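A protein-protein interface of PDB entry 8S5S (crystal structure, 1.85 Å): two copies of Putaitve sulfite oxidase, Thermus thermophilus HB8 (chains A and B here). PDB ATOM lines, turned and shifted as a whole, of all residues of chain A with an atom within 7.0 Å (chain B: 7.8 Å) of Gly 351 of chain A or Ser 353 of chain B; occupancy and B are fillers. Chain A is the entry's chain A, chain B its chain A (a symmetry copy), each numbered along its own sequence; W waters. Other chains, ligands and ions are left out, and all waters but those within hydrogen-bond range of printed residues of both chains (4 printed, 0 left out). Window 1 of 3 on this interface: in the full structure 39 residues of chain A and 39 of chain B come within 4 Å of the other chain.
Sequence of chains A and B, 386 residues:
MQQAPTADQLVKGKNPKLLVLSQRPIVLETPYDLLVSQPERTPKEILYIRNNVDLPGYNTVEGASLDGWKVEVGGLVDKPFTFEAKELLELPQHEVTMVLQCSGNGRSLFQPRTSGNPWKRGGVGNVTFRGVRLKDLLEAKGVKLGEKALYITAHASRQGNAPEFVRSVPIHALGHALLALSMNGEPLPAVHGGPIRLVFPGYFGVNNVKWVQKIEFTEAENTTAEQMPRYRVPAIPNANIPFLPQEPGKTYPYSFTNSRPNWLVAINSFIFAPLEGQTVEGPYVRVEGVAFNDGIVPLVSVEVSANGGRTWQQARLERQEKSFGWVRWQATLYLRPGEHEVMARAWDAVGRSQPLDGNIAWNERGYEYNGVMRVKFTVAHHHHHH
Of the printed residues of chain B, Ala 349 of chain A touches Pro 355 and Ile 360.
Gly 351 of chain A touches just these residues of chain B: Ser 353, Gln 354 and Pro 355.
Of chain A, only Trp 347 and Gly 351 come within 4 Å of Ser 353 of chain B.
Of the printed residues of chain A, Gln 354 of chain B touches Trp 347 and Gly 351.
Among the printed residues, merely in contact across the chains: Arg 345 of chain A with Trp 347 of chain B (3.2 Å), Trp 347 of chain A with Arg 345 of chain B (3.2 Å), Ala 349 of chain A with Pro 355 of chain B (3.2 Å), Ala 349 of chain A with Ile 360 of chain B (3.3 Å), Val 350 of chain A with Phe 243 of chain B (3.5 Å), Gln 354 of chain A with Gly 351 of chain B (3.6 Å), Gly 351 of chain A with Gln 354 of chain B (3.6 Å), Gly 351 of chain A with Pro 355 of chain B (3.6 Å), Val 300 of chain A with Leu 356 of chain B (3.7 Å), Arg 352 of chain A with Pro 242 of chain B (3.7 Å), Trp 347 of chain A with Leu 356 of chain B (3.7 Å), Ser 353 of chain A with Trp 347 of chain B (3.7 Å), Trp 347 of chain A with Ser 353 of chain B (3.7 Å) and Val 350 of chain A with Pro 242 of chain B (3.8 Å).
O of Gln 354 of chain A lies within hydrogen-bond range of NE1 of Trp 347 of chain B (2.9 Å).
NH2 of Arg 345 of chain A lies within salt-bridge range of OE1 of Glu 303 of chain B (2.9 Å).
The guanidinium group (NH2) of Arg 345 of chain A sits close to the guanidinium group (NH2) of Arg 345 of chain B.
The backbone carbonyl oxygen (O) of Gly 351 of chain B is in hydrogen-bond range of the backbone NH (N) of Ser 353 of chain A.
The backbone carbonyl oxygen of Gly 351 of chain A lies within hydrogen-bond range of the backbone NH of Ser 353 of chain B (2.9 Å).
NE1 of Trp 347 of chain A lies within hydrogen-bond range of O of Gln 354 of chain B.
Water W1 lies within hydrogen-bond range of the backbone carbonyl oxygen of Ala 349 of chain A (2.6 Å) and the backbone NH of Asp 357 of chain B (3.0 Å).
Water W3 bridges the backbone carbonyl oxygen of Asp 348 of chain A and the backbone NH of Leu 356 of chain B.
Water W4 bridges O of Ser 353 of chain B and O of Val 350 of chain A.
Water W2 bridges O of Ser 353 of chain A (2.8 Å) and O of Val 350 of chain B (2.9 Å).
The backbone NH of Gly 351 of chain B sits at hydrogen-bond distance from the side-chain carboxylate of Asp 348 of chain B, 3.3 Å away.
The side-chain carboxylate (OD1) of Asp 348 of chain A sits at hydrogen-bond distance from the backbone NH (N) of Gly 351 of chain A.
OG of Ser 301 of chain B lies within hydrogen-bond range of OE2 of Glu 303 of chain B, at 2.7 Å.
The backbone NH (N) of Val 350 of chain A sits close to the side-chain carboxylate (OD1) of Asp 348 of chain A (3.1 Å).
Of the 13 printed residues of chain A, 9 touch a printed residue of chain B.
Printed residues of chain A that touch a printed residue of chain B: Val 300, Arg 345, Trp 347, Ala 349, Val 350, Gly 351, Arg 352, Ser 353 and Gln 354.
Hydrophobic or aromatic side chains of chain A that line the printed part of chain B: Val 300, Trp 347, Ala 349 and Val 350.
Of the 23 printed residues of chain B, 11 touch a printed residue of chain A.
Hydrophobic or aromatic side chains of chain B that line the printed part of chain A: Pro 242, Phe 243, Trp 347, Pro 355, Leu 356 and Ile 360.
Among the printed residues, Asp or Glu carboxylates within 4 Å of a Lys or Arg side-chain nitrogen of the other chain: Arg 345 of chain A with Glu 303 of chain B.
Trp 347 of chain A touches Ser 353 of chain B, and with the chains exchanged Ser 353 of chain A touches Trp 347 of chain B.
Gly 351 of chain A touches Gln 354 of chain B, and with the chains exchanged Gln 354 of chain A touches Gly 351 of chain B.
Positions printed for both chains: 267, 345, 346, 347, 348, 350, 351, 352, 353 and 354.
Of the 20 pairs that touch across the chains among the printed residues, 11 have their exchanged pair printed and touching as well.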
ATOM      1  N   ILE A 267     -13.267   2.565  22.737  1.00  0.00           N
ATOM      2  CA  ILE A 267     -14.409   2.415  21.837  1.00  0.00           C
ATOM      3  C   ILE A 267     -14.567   3.710  21.025  1.00  0.00           C
ATOM      4  O   ILE A 267     -14.333   4.800  21.524  1.00  0.00           O
ATOM      5  CB  ILE A 267     -15.690   2.075  22.617  1.00  0.00           C
ATOM      6  CG1 ILE A 267     -16.810   1.728  21.690  1.00  0.00           C
ATOM      7  CG2 ILE A 267     -16.064   3.168  23.611  1.00  0.00           C
ATOM      8  CD1 ILE A 267     -18.006   1.118  22.388  1.00  0.00           C
ATOM      9  N   VAL A 297     -15.767  -7.828  23.435  1.00  0.00           N
ATOM     10  CA  VAL A 297     -17.196  -8.064  23.361  1.00  0.00           C
ATOM     11  C   VAL A 297     -17.695  -7.394  22.106  1.00  0.00           C
ATOM     12  O   VAL A 297     -17.042  -6.507  21.582  1.00  0.00           O
ATOM     13  CB  VAL A 297     -18.000  -7.554  24.575  1.00  0.00           C
ATOM     14  CG1 VAL A 297     -17.479  -8.208  25.839  1.00  0.00           C
ATOM     15  CG2 VAL A 297     -17.938  -6.036  24.726  1.00  0.00           C
ATOM     16  N   VAL A 300     -22.990  -3.288  20.441  1.00  0.00           N
ATOM     17  CA  VAL A 300     -24.438  -3.405  20.457  1.00  0.00           C
ATOM     18  C   VAL A 300     -25.092  -2.449  19.469  1.00  0.00           C
ATOM     19  O   VAL A 300     -26.030  -2.844  18.770  1.00  0.00           O
ATOM     20  CB  VAL A 300     -24.989  -3.222  21.879  1.00  0.00           C
ATOM     21  CG1 VAL A 300     -26.509  -2.961  21.859  1.00  0.00           C
ATOM     22  CG2 VAL A 300     -24.690  -4.473  22.698  1.00  0.00           C
ATOM     23  N   ARG A 345     -22.099   7.719  17.810  1.00  0.00           N
ATOM     24  CA  ARG A 345     -21.744   7.186  19.112  1.00  0.00           C
ATOM     25  C   ARG A 345     -21.827   5.673  19.055  1.00  0.00           C
ATOM     26  O   ARG A 345     -22.854   5.131  18.670  1.00  0.00           O
ATOM     27  CB  ARG A 345     -22.755   7.703  20.142  1.00  0.00           C
ATOM     28  CG  ARG A 345     -22.553   7.297  21.585  1.00  0.00           C
ATOM     29  CD  ARG A 345     -23.678   7.834  22.539  1.00  0.00           C
ATOM     30  NE  ARG A 345     -25.024   7.394  22.164  1.00  0.00           N
ATOM     31  CZ  ARG A 345     -26.103   7.906  22.729  1.00  0.00           C
ATOM     32  NH1 ARG A 345     -25.994   8.846  23.651  1.00  0.00           N
ATOM     33  NH2 ARG A 345     -27.294   7.483  22.410  1.00  0.00           N
ATOM     34  N   ALA A 346     -20.767   4.981  19.488  1.00  0.00           N
ATOM     35  CA  ALA A 346     -20.809   3.532  19.588  1.00  0.00           C
ATOM     36  C   ALA A 346     -21.142   3.110  21.024  1.00  0.00           C
ATOM     37  O   ALA A 346     -20.765   3.834  21.968  1.00  0.00           O
ATOM     38  CB  ALA A 346     -19.449   2.996  19.167  1.00  0.00           C
ATOM     39  N   TRP A 347     -21.701   1.907  21.171  1.00  0.00           N
ATOM     40  CA  TRP A 347     -22.144   1.349  22.439  1.00  0.00           C
ATOM     41  C   TRP A 347     -21.935  -0.152  22.410  1.00  0.00           C
ATOM     42  O   TRP A 347     -22.442  -0.831  21.522  1.00  0.00           O
ATOM     43  CB  TRP A 347     -23.618   1.686  22.682  1.00  0.00           C
ATOM     44  CG  TRP A 347     -24.242   1.326  23.994  1.00  0.00           C
ATOM     45  CD1 TRP A 347     -23.744   1.413  25.263  1.00  0.00           C
ATOM     46  CD2 TRP A 347     -25.610   0.887  24.133  1.00  0.00           C
ATOM     47  NE1 TRP A 347     -24.703   1.020  26.168  1.00  0.00           N
ATOM     48  CE2 TRP A 347     -25.843   0.681  25.505  1.00  0.00           C
ATOM     49  CE3 TRP A 347     -26.641   0.612  23.213  1.00  0.00           C
ATOM     50  CZ2 TRP A 347     -27.088   0.267  25.985  1.00  0.00           C
ATOM     51  CZ3 TRP A 347     -27.842   0.154  23.686  1.00  0.00           C
ATOM     52  CH2 TRP A 347     -28.065   0.006  25.056  1.00  0.00           C
ATOM     53  N   ASP A 348     -21.186  -0.679  23.374  1.00  0.00           N
ATOM     54  CA  ASP A 348     -20.862  -2.102  23.299  1.00  0.00           C
ATOM     55  C   ASP A 348     -21.572  -2.880  24.404  1.00  0.00           C
ATOM     56  O   ASP A 348     -22.245  -2.303  25.264  1.00  0.00           O
ATOM     57  CB  ASP A 348     -19.371  -2.335  23.193  1.00  0.00           C
ATOM     58  CG  ASP A 348     -18.590  -2.274  24.494  1.00  0.00           C
ATOM     59  OD1 ASP A 348     -19.241  -2.143  25.548  1.00  0.00           O
ATOM     60  OD2 ASP A 348     -17.348  -2.352  24.400  1.00  0.00           O
ATOM     61  N   ALA A 349     -21.396  -4.189  24.354  1.00  0.00           N
ATOM     62  CA  ALA A 349     -22.226  -5.107  25.124  1.00  0.00           C
ATOM     63  C   ALA A 349     -21.982  -4.967  26.622  1.00  0.00           C
ATOM     64  O   ALA A 349     -22.803  -5.441  27.443  1.00  0.00           O
ATOM     65  CB  ALA A 349     -21.955  -6.496  24.640  1.00  0.00           C
ATOM     66  N   VAL A 350     -20.815  -4.417  27.007  1.00  0.00           N
ATOM     67  CA  VAL A 350     -20.546  -4.244  28.438  1.00  0.00           C
ATOM     68  C   VAL A 350     -20.898  -2.823  28.882  1.00  0.00           C
ATOM     69  O   VAL A 350     -20.765  -2.486  30.060  1.00  0.00           O
ATOM     70  CB  VAL A 350     -19.135  -4.604  28.939  1.00  0.00           C
ATOM     71  CG1 VAL A 350     -18.831  -6.080  28.769  1.00  0.00           C
ATOM     72  CG2 VAL A 350     -18.065  -3.728  28.306  1.00  0.00           C
ATOM     73  N   GLY A 351     -21.428  -2.012  27.984  1.00  0.00           N
ATOM     74  CA  GLY A 351     -21.943  -0.723  28.402  1.00  0.00           C
ATOM     75  C   GLY A 351     -20.986   0.410  28.071  1.00  0.00           C
ATOM     76  O   GLY A 351     -21.292   1.556  28.390  1.00  0.00           O
ATOM     77  N   ARG A 352     -19.834   0.114  27.465  1.00  0.00           N
ATOM     78  CA  ARG A 352     -18.887   1.196  27.195  1.00  0.00           C
ATOM     79  C   ARG A 352     -19.494   2.053  26.091  1.00  0.00           C
ATOM     80  O   ARG A 352     -20.146   1.545  25.165  1.00  0.00           O
ATOM     81  CB  ARG A 352     -17.536   0.633  26.752  1.00  0.00           C
ATOM     82  CG  ARG A 352     -16.752   0.053  27.914  1.00  0.00           C
ATOM     83  CD  ARG A 352     -15.433  -0.601  27.502  1.00  0.00           C
ATOM     84  NE  ARG A 352     -15.510  -1.647  26.487  1.00  0.00           N
ATOM     85  CZ  ARG A 352     -14.548  -2.487  26.174  1.00  0.00           C
ATOM     86  NH1 ARG A 352     -13.367  -2.407  26.758  1.00  0.00           N
ATOM     87  NH2 ARG A 352     -14.786  -3.463  25.327  1.00  0.00           N
ATOM     88  N   SER A 353     -19.225   3.352  26.156  1.00  0.00           N
ATOM     89  CA  SER A 353     -19.571   4.249  25.070  1.00  0.00           C
ATOM     90  C   SER A 353     -18.544   5.378  25.019  1.00  0.00           C
ATOM     91  O   SER A 353     -17.511   5.328  25.699  1.00  0.00           O
ATOM     92  CB  SER A 353     -20.965   4.755  25.214  1.00  0.00           C
ATOM     93  OG  SER A 353     -21.457   5.425  24.056  1.00  0.00           O
ATOM     94  N   GLN A 354     -18.829   6.417  24.260  1.00  0.00           N
ATOM     95  CA  GLN A 354     -17.869   7.485  24.044  1.00  0.00           C
ATOM     96  C   GLN A 354     -18.293   8.742  24.807  1.00  0.00           C
ATOM     97  O   GLN A 354     -19.474   9.002  24.965  1.00  0.00           O
ATOM     98  CB  GLN A 354     -17.832   7.809  22.539  1.00  0.00           C
ATOM     99  CG  GLN A 354     -17.419   6.665  21.637  1.00  0.00           C
ATOM    100  CD  GLN A 354     -17.592   7.004  20.180  1.00  0.00           C
ATOM    101  OE1 GLN A 354     -18.427   6.440  19.483  1.00  0.00           O
ATOM    102  NE2 GLN A 354     -16.827   7.997  19.738  1.00  0.00           N
ATOM    103  N   PRO B 242     -15.020  -2.460  31.979  1.00  0.00           N
ATOM    104  CA  PRO B 242     -15.672  -2.516  33.286  1.00  0.00           C
ATOM    105  C   PRO B 242     -15.576  -3.847  34.024  1.00  0.00           C
ATOM    106  O   PRO B 242     -15.532  -3.862  35.234  1.00  0.00           O
ATOM    107  CB  PRO B 242     -17.129  -2.148  33.029  1.00  0.00           C
ATOM    108  CG  PRO B 242     -17.197  -1.843  31.565  1.00  0.00           C
ATOM    109  CD  PRO B 242     -15.874  -1.928  30.908  1.00  0.00           C
ATOM    110  N   PHE B 243     -15.550  -4.936  33.266  1.00  0.00           N
ATOM    111  CA  PHE B 243     -15.334  -6.266  33.792  1.00  0.00           C
ATOM    112  C   PHE B 243     -15.004  -7.152  32.600  1.00  0.00           C
ATOM    113  O   PHE B 243     -15.285  -6.775  31.454  1.00  0.00           O
ATOM    114  CB  PHE B 243     -16.616  -6.714  34.524  1.00  0.00           C
ATOM    115  CG  PHE B 243     -17.866  -6.572  33.685  1.00  0.00           C
ATOM    116  CD1 PHE B 243     -18.231  -7.553  32.779  1.00  0.00           C
ATOM    117  CD2 PHE B 243     -18.681  -5.445  33.812  1.00  0.00           C
ATOM    118  CE1 PHE B 243     -19.366  -7.385  32.004  1.00  0.00           C
ATOM    119  CE2 PHE B 243     -19.750  -5.235  32.971  1.00  0.00           C
ATOM    120  CZ  PHE B 243     -20.117  -6.229  32.084  1.00  0.00           C
ATOM    121  N   ALA B 266     -21.752   1.347  39.937  1.00  0.00           N
ATOM    122  CA  ALA B 266     -21.921   1.216  38.494  1.00  0.00           C
ATOM    123  C   ALA B 266     -23.017   2.170  38.051  1.00  0.00           C
ATOM    124  O   ALA B 266     -24.046   2.291  38.721  1.00  0.00           O
ATOM    125  CB  ALA B 266     -22.291  -0.203  38.108  1.00  0.00           C
ATOM    126  N   ILE B 267     -22.819   2.795  36.898  1.00  0.00           N
ATOM    127  CA  ILE B 267     -23.787   3.750  36.362  1.00  0.00           C
ATOM    128  C   ILE B 267     -25.127   3.026  36.155  1.00  0.00           C
ATOM    129  O   ILE B 267     -25.165   1.861  35.789  1.00  0.00           O
ATOM    130  CB  ILE B 267     -23.278   4.384  35.057  1.00  0.00           C
ATOM    131  CG1 ILE B 267     -24.170   5.499  34.615  1.00  0.00           C
ATOM    132  CG2 ILE B 267     -23.045   3.345  33.967  1.00  0.00           C
ATOM    133  CD1 ILE B 267     -23.580   6.340  33.505  1.00  0.00           C
ATOM    134  N   ASN B 268     -26.231   3.707  36.430  1.00  0.00           N
ATOM    135  CA  ASN B 268     -27.506   3.004  36.421  1.00  0.00           C
ATOM    136  C   ASN B 268     -28.629   4.007  36.214  1.00  0.00           C
ATOM    137  O   ASN B 268     -28.472   5.205  36.449  1.00  0.00           O
ATOM    138  CB  ASN B 268     -27.640   2.231  37.737  1.00  0.00           C
ATOM    139  CG  ASN B 268     -28.398   0.939  37.590  1.00  0.00           C
ATOM    140  OD1 ASN B 268     -29.275   0.811  36.725  1.00  0.00           O
ATOM    141  ND2 ASN B 268     -28.073  -0.024  38.441  1.00  0.00           N
ATOM    142  N   SER B 301     -26.614  12.341  29.926  1.00  0.00           N
ATOM    143  CA  SER B 301     -27.987  12.132  29.544  1.00  0.00           C
ATOM    144  C   SER B 301     -28.566  10.905  30.235  1.00  0.00           C
ATOM    145  O   SER B 301     -27.858   9.975  30.614  1.00  0.00           O
ATOM    146  CB  SER B 301     -28.170  12.045  28.063  1.00  0.00           C
ATOM    147  OG  SER B 301     -27.772  10.762  27.583  1.00  0.00           O
ATOM    148  N   GLU B 303     -31.625   8.466  28.623  1.00  0.00           N
ATOM    149  CA  GLU B 303     -32.357   8.336  27.375  1.00  0.00           C
ATOM    150  C   GLU B 303     -33.344   7.212  27.514  1.00  0.00           C
ATOM    151  O   GLU B 303     -33.102   6.247  28.234  1.00  0.00           O
ATOM    152  CB  GLU B 303     -31.453   8.159  26.159  1.00  0.00           C
ATOM    153  CG  GLU B 303     -30.472   9.324  26.029  1.00  0.00           C
ATOM    154  CD  GLU B 303     -29.335   9.085  25.053  1.00  0.00           C
ATOM    155  OE1 GLU B 303     -29.445   8.135  24.245  1.00  0.00           O
ATOM    156  OE2 GLU B 303     -28.364   9.871  25.077  1.00  0.00           O
ATOM    157  N   ALA B 344     -34.615   2.497  29.866  1.00  0.00           N
ATOM    158  CA  ALA B 344     -33.877   3.692  30.201  1.00  0.00           C
ATOM    159  C   ALA B 344     -32.376   3.381  30.290  1.00  0.00           C
ATOM    160  O   ALA B 344     -31.979   2.287  30.702  1.00  0.00           O
ATOM    161  CB  ALA B 344     -34.337   4.318  31.487  1.00  0.00           C
ATOM    162  N   ARG B 345     -31.579   4.354  29.851  1.00  0.00           N
ATOM    163  CA  ARG B 345     -30.138   4.203  29.772  1.00  0.00           C
ATOM    164  C   ARG B 345     -29.489   5.500  30.214  1.00  0.00           C
ATOM    165  O   ARG B 345     -29.807   6.554  29.683  1.00  0.00           O
ATOM    166  CB  ARG B 345     -29.758   3.926  28.312  1.00  0.00           C
ATOM    167  CG  ARG B 345     -28.296   3.697  28.002  1.00  0.00           C
ATOM    168  CD  ARG B 345     -28.016   3.483  26.472  1.00  0.00           C
ATOM    169  NE  ARG B 345     -28.452   4.603  25.635  1.00  0.00           N
ATOM    170  CZ  ARG B 345     -28.479   4.512  24.316  1.00  0.00           C
ATOM    171  NH1 ARG B 345     -28.119   3.393  23.714  1.00  0.00           N
ATOM    172  NH2 ARG B 345     -28.837   5.527  23.581  1.00  0.00           N
ATOM    173  N   ALA B 346     -28.538   5.423  31.150  1.00  0.00           N
ATOM    174  CA  ALA B 346     -27.774   6.597  31.541  1.00  0.00           C
ATOM    175  C   ALA B 346     -26.441   6.637  30.786  1.00  0.00           C
ATOM    176  O   ALA B 346     -25.894   5.561  30.470  1.00  0.00           O
ATOM    177  CB  ALA B 346     -27.547   6.527  33.043  1.00  0.00           C
ATOM    178  N   TRP B 347     -25.881   7.840  30.639  1.00  0.00           N
ATOM    179  CA  TRP B 347     -24.652   8.098  29.907  1.00  0.00           C
ATOM    180  C   TRP B 347     -23.913   9.237  30.580  1.00  0.00           C
ATOM    181  O   TRP B 347     -24.466  10.321  30.747  1.00  0.00           O
ATOM    182  CB  TRP B 347     -24.964   8.442  28.447  1.00  0.00           C
ATOM    183  CG  TRP B 347     -23.834   8.610  27.479  1.00  0.00           C
ATOM    184  CD1 TRP B 347     -22.682   7.892  27.335  1.00  0.00           C
ATOM    185  CD2 TRP B 347     -23.841   9.573  26.405  1.00  0.00           C
ATOM    186  NE1 TRP B 347     -21.962   8.376  26.267  1.00  0.00           N
ATOM    187  CE2 TRP B 347     -22.640   9.409  25.692  1.00  0.00           C
ATOM    188  CE3 TRP B 347     -24.740  10.584  26.011  1.00  0.00           C
ATOM    189  CZ2 TRP B 347     -22.339  10.184  24.570  1.00  0.00           C
ATOM    190  CZ3 TRP B 347     -24.414  11.376  24.942  1.00  0.00           C
ATOM    191  CH2 TRP B 347     -23.239  11.162  24.221  1.00  0.00           C
ATOM    192  N   ASP B 348     -22.666   9.003  30.976  1.00  0.00           N
ATOM    193  CA  ASP B 348     -21.976  10.037  31.741  1.00  0.00           C
ATOM    194  C   ASP B 348     -20.844  10.655  30.923  1.00  0.00           C
ATOM    195  O   ASP B 348     -20.554  10.224  29.803  1.00  0.00           O
ATOM    196  CB  ASP B 348     -21.592   9.555  33.123  1.00  0.00           C
ATOM    197  CG  ASP B 348     -20.330   8.715  33.212  1.00  0.00           C
ATOM    198  OD1 ASP B 348     -19.659   8.577  32.172  1.00  0.00           O
ATOM    199  OD2 ASP B 348     -20.071   8.220  34.328  1.00  0.00           O
ATOM    200  N   VAL B 350     -17.728  10.714  30.956  1.00  0.00           N
ATOM    201  CA  VAL B 350     -16.535   9.983  30.522  1.00  0.00           C
ATOM    202  C   VAL B 350     -16.918   8.842  29.576  1.00  0.00           C
ATOM    203  O   VAL B 350     -16.048   8.123  29.080  1.00  0.00           O
ATOM    204  CB  VAL B 350     -15.596   9.447  31.619  1.00  0.00           C
ATOM    205  CG1 VAL B 350     -14.966  10.565  32.425  1.00  0.00           C
ATOM    206  CG2 VAL B 350     -16.288   8.426  32.510  1.00  0.00           C
ATOM    207  N   GLY B 351     -18.192   8.720  29.247  1.00  0.00           N
ATOM    208  CA  GLY B 351     -18.574   7.773  28.217  1.00  0.00           C
ATOM    209  C   GLY B 351     -19.159   6.498  28.802  1.00  0.00           C
ATOM    210  O   GLY B 351     -19.508   5.603  28.037  1.00  0.00           O
ATOM    211  N   ARG B 352     -19.252   6.390  30.128  1.00  0.00           N
ATOM    212  CA  ARG B 352     -19.764   5.142  30.695  1.00  0.00           C
ATOM    213  C   ARG B 352     -21.252   5.085  30.373  1.00  0.00           C
ATOM    214  O   ARG B 352     -21.952   6.109  30.378  1.00  0.00           O
ATOM    215  CB  ARG B 352     -19.543   5.105  32.208  1.00  0.00           C
ATOM    216  CG  ARG B 352     -18.095   4.833  32.566  1.00  0.00           C
ATOM    217  CD  ARG B 352     -17.811   4.876  34.067  1.00  0.00           C
ATOM    218  NE  ARG B 352     -18.193   6.096  34.771  1.00  0.00           N
ATOM    219  CZ  ARG B 352     -17.826   6.429  35.988  1.00  0.00           C
ATOM    220  NH1 ARG B 352     -17.083   5.616  36.715  1.00  0.00           N
ATOM    221  NH2 ARG B 352     -18.137   7.615  36.461  1.00  0.00           N
ATOM    222  N   SER B 353     -21.748   3.872  30.154  1.00  0.00           N
ATOM    223  CA  SER B 353     -23.175   3.653  30.032  1.00  0.00           C
ATOM    224  C   SER B 353     -23.505   2.257  30.557  1.00  0.00           C
ATOM    225  O   SER B 353     -22.655   1.589  31.160  1.00  0.00           O
ATOM    226  CB  SER B 353     -23.633   3.853  28.627  1.00  0.00           C
ATOM    227  OG  SER B 353     -25.051   3.912  28.486  1.00  0.00           O
ATOM    228  N   GLN B 354     -24.710   1.787  30.303  1.00  0.00           N
ATOM    229  CA  GLN B 354     -25.167   0.526  30.861  1.00  0.00           C
ATOM    230  C   GLN B 354     -25.220  -0.548  29.774  1.00  0.00           C
ATOM    231  O   GLN B 354     -25.496  -0.252  28.623  1.00  0.00           O
ATOM    232  CB  GLN B 354     -26.584   0.730  31.427  1.00  0.00           C
ATOM    233  CG  GLN B 354     -26.704   1.762  32.528  1.00  0.00           C
ATOM    234  CD  GLN B 354     -28.140   2.036  32.890  1.00  0.00           C
ATOM    235  OE1 GLN B 354     -28.665   3.120  32.661  1.00  0.00           O
ATOM    236  NE2 GLN B 354     -28.799   1.003  33.404  1.00  0.00           N
ATOM    237  N   PRO B 355     -24.977  -1.833  30.072  1.00  0.00           N
ATOM    238  CA  PRO B 355     -25.146  -2.905  29.084  1.00  0.00           C
ATOM    239  C   PRO B 355     -26.621  -3.087  28.740  1.00  0.00           C
ATOM    240  O   PRO B 355     -27.473  -3.008  29.625  1.00  0.00           O
ATOM    241  CB  PRO B 355     -24.610  -4.162  29.786  1.00  0.00           C
ATOM    242  CG  PRO B 355     -24.737  -3.824  31.190  1.00  0.00           C
ATOM    243  CD  PRO B 355     -24.547  -2.322  31.384  1.00  0.00           C
ATOM    244  N   LEU B 356     -26.908  -3.337  27.473  1.00  0.00           N
ATOM    245  CA  LEU B 356     -28.264  -3.593  27.038  1.00  0.00           C
ATOM    246  C   LEU B 356     -28.784  -4.874  27.697  1.00  0.00           C
ATOM    247  O   LEU B 356     -29.923  -4.940  28.139  1.00  0.00           O
ATOM    248  CB  LEU B 356     -28.325  -3.673  25.513  1.00  0.00           C
ATOM    249  CG  LEU B 356     -29.695  -4.033  24.921  1.00  0.00           C
ATOM    250  CD1 LEU B 356     -30.735  -3.005  25.276  1.00  0.00           C
ATOM    251  CD2 LEU B 356     -29.623  -4.125  23.403  1.00  0.00           C
ATOM    252  N   ASP B 357     -27.953  -5.903  27.740  1.00  0.00           N
ATOM    253  CA  ASP B 357     -28.265  -7.140  28.457  1.00  0.00           C
ATOM    254  C   ASP B 357     -27.352  -7.261  29.682  1.00  0.00           C
ATOM    255  O   ASP B 357     -26.171  -7.633  29.564  1.00  0.00           O
ATOM    256  CB  ASP B 357     -28.119  -8.338  27.530  1.00  0.00           C
ATOM    257  CG  ASP B 357     -28.401  -9.692  28.178  1.00  0.00           C
ATOM    258  OD1 ASP B 357     -28.708  -9.736  29.382  1.00  0.00           O
ATOM    259  OD2 ASP B 357     -28.261 -10.707  27.485  1.00  0.00           O
ATOM    260  N   ILE B 360     -24.612 -10.140  30.670  1.00  0.00           N
ATOM    261  CA  ILE B 360     -23.238 -10.281  30.185  1.00  0.00           C
ATOM    262  C   ILE B 360     -22.243 -10.222  31.368  1.00  0.00           C
ATOM    263  O   ILE B 360     -21.133 -10.782  31.313  1.00  0.00           O
ATOM    264  CB  ILE B 360     -22.931  -9.211  29.120  1.00  0.00           C
ATOM    265  CG1 ILE B 360     -21.623  -9.532  28.366  1.00  0.00           C
ATOM    266  CG2 ILE B 360     -22.883  -7.822  29.757  1.00  0.00           C
ATOM    267  CD1 ILE B 360     -21.467  -8.794  27.052  1.00  0.00           C
ATOM    268  N   ASN B 370     -26.253  -3.899  36.345  1.00  0.00           N
ATOM    269  CA  ASN B 370     -26.651  -2.568  35.943  1.00  0.00           C
ATOM    270  C   ASN B 370     -27.204  -2.542  34.528  1.00  0.00           C
ATOM    271  O   ASN B 370     -27.127  -1.521  33.834  1.00  0.00           O
ATOM    272  CB  ASN B 370     -25.524  -1.552  36.092  1.00  0.00           C
ATOM    273  CG  ASN B 370     -24.482  -1.688  35.012  1.00  0.00           C
ATOM    274  OD1 ASN B 370     -24.201  -2.773  34.488  1.00  0.00           O
ATOM    275  ND2 ASN B 370     -23.845  -0.575  34.713  1.00  0.00           N
ATOM    276  N   VAL B 372     -29.715  -2.263  31.447  1.00  0.00           N
ATOM    277  CA  VAL B 372     -30.850  -1.430  31.079  1.00  0.00           C
ATOM    278  C   VAL B 372     -32.172  -1.972  31.640  1.00  0.00           C
ATOM    279  O   VAL B 372     -32.565  -3.105  31.369  1.00  0.00           O
ATOM    280  CB  VAL B 372     -30.859  -1.320  29.555  1.00  0.00           C
ATOM    281  CG1 VAL B 372     -32.221  -0.908  28.988  1.00  0.00           C
ATOM    282  CG2 VAL B 372     -29.783  -0.338  29.153  1.00  0.00           C
HETATM  283  O   HOH W   1     -25.168  -6.483  26.952  1.00  0.00           O
HETATM  284  O   HOH W   2     -15.210   6.171  27.126  1.00  0.00           O
HETATM  285  O   HOH W   3     -25.035  -2.461  25.438  1.00  0.00           O
HETATM  286  O   HOH W   4     -21.289  -0.654  32.229  1.00  0.00           O
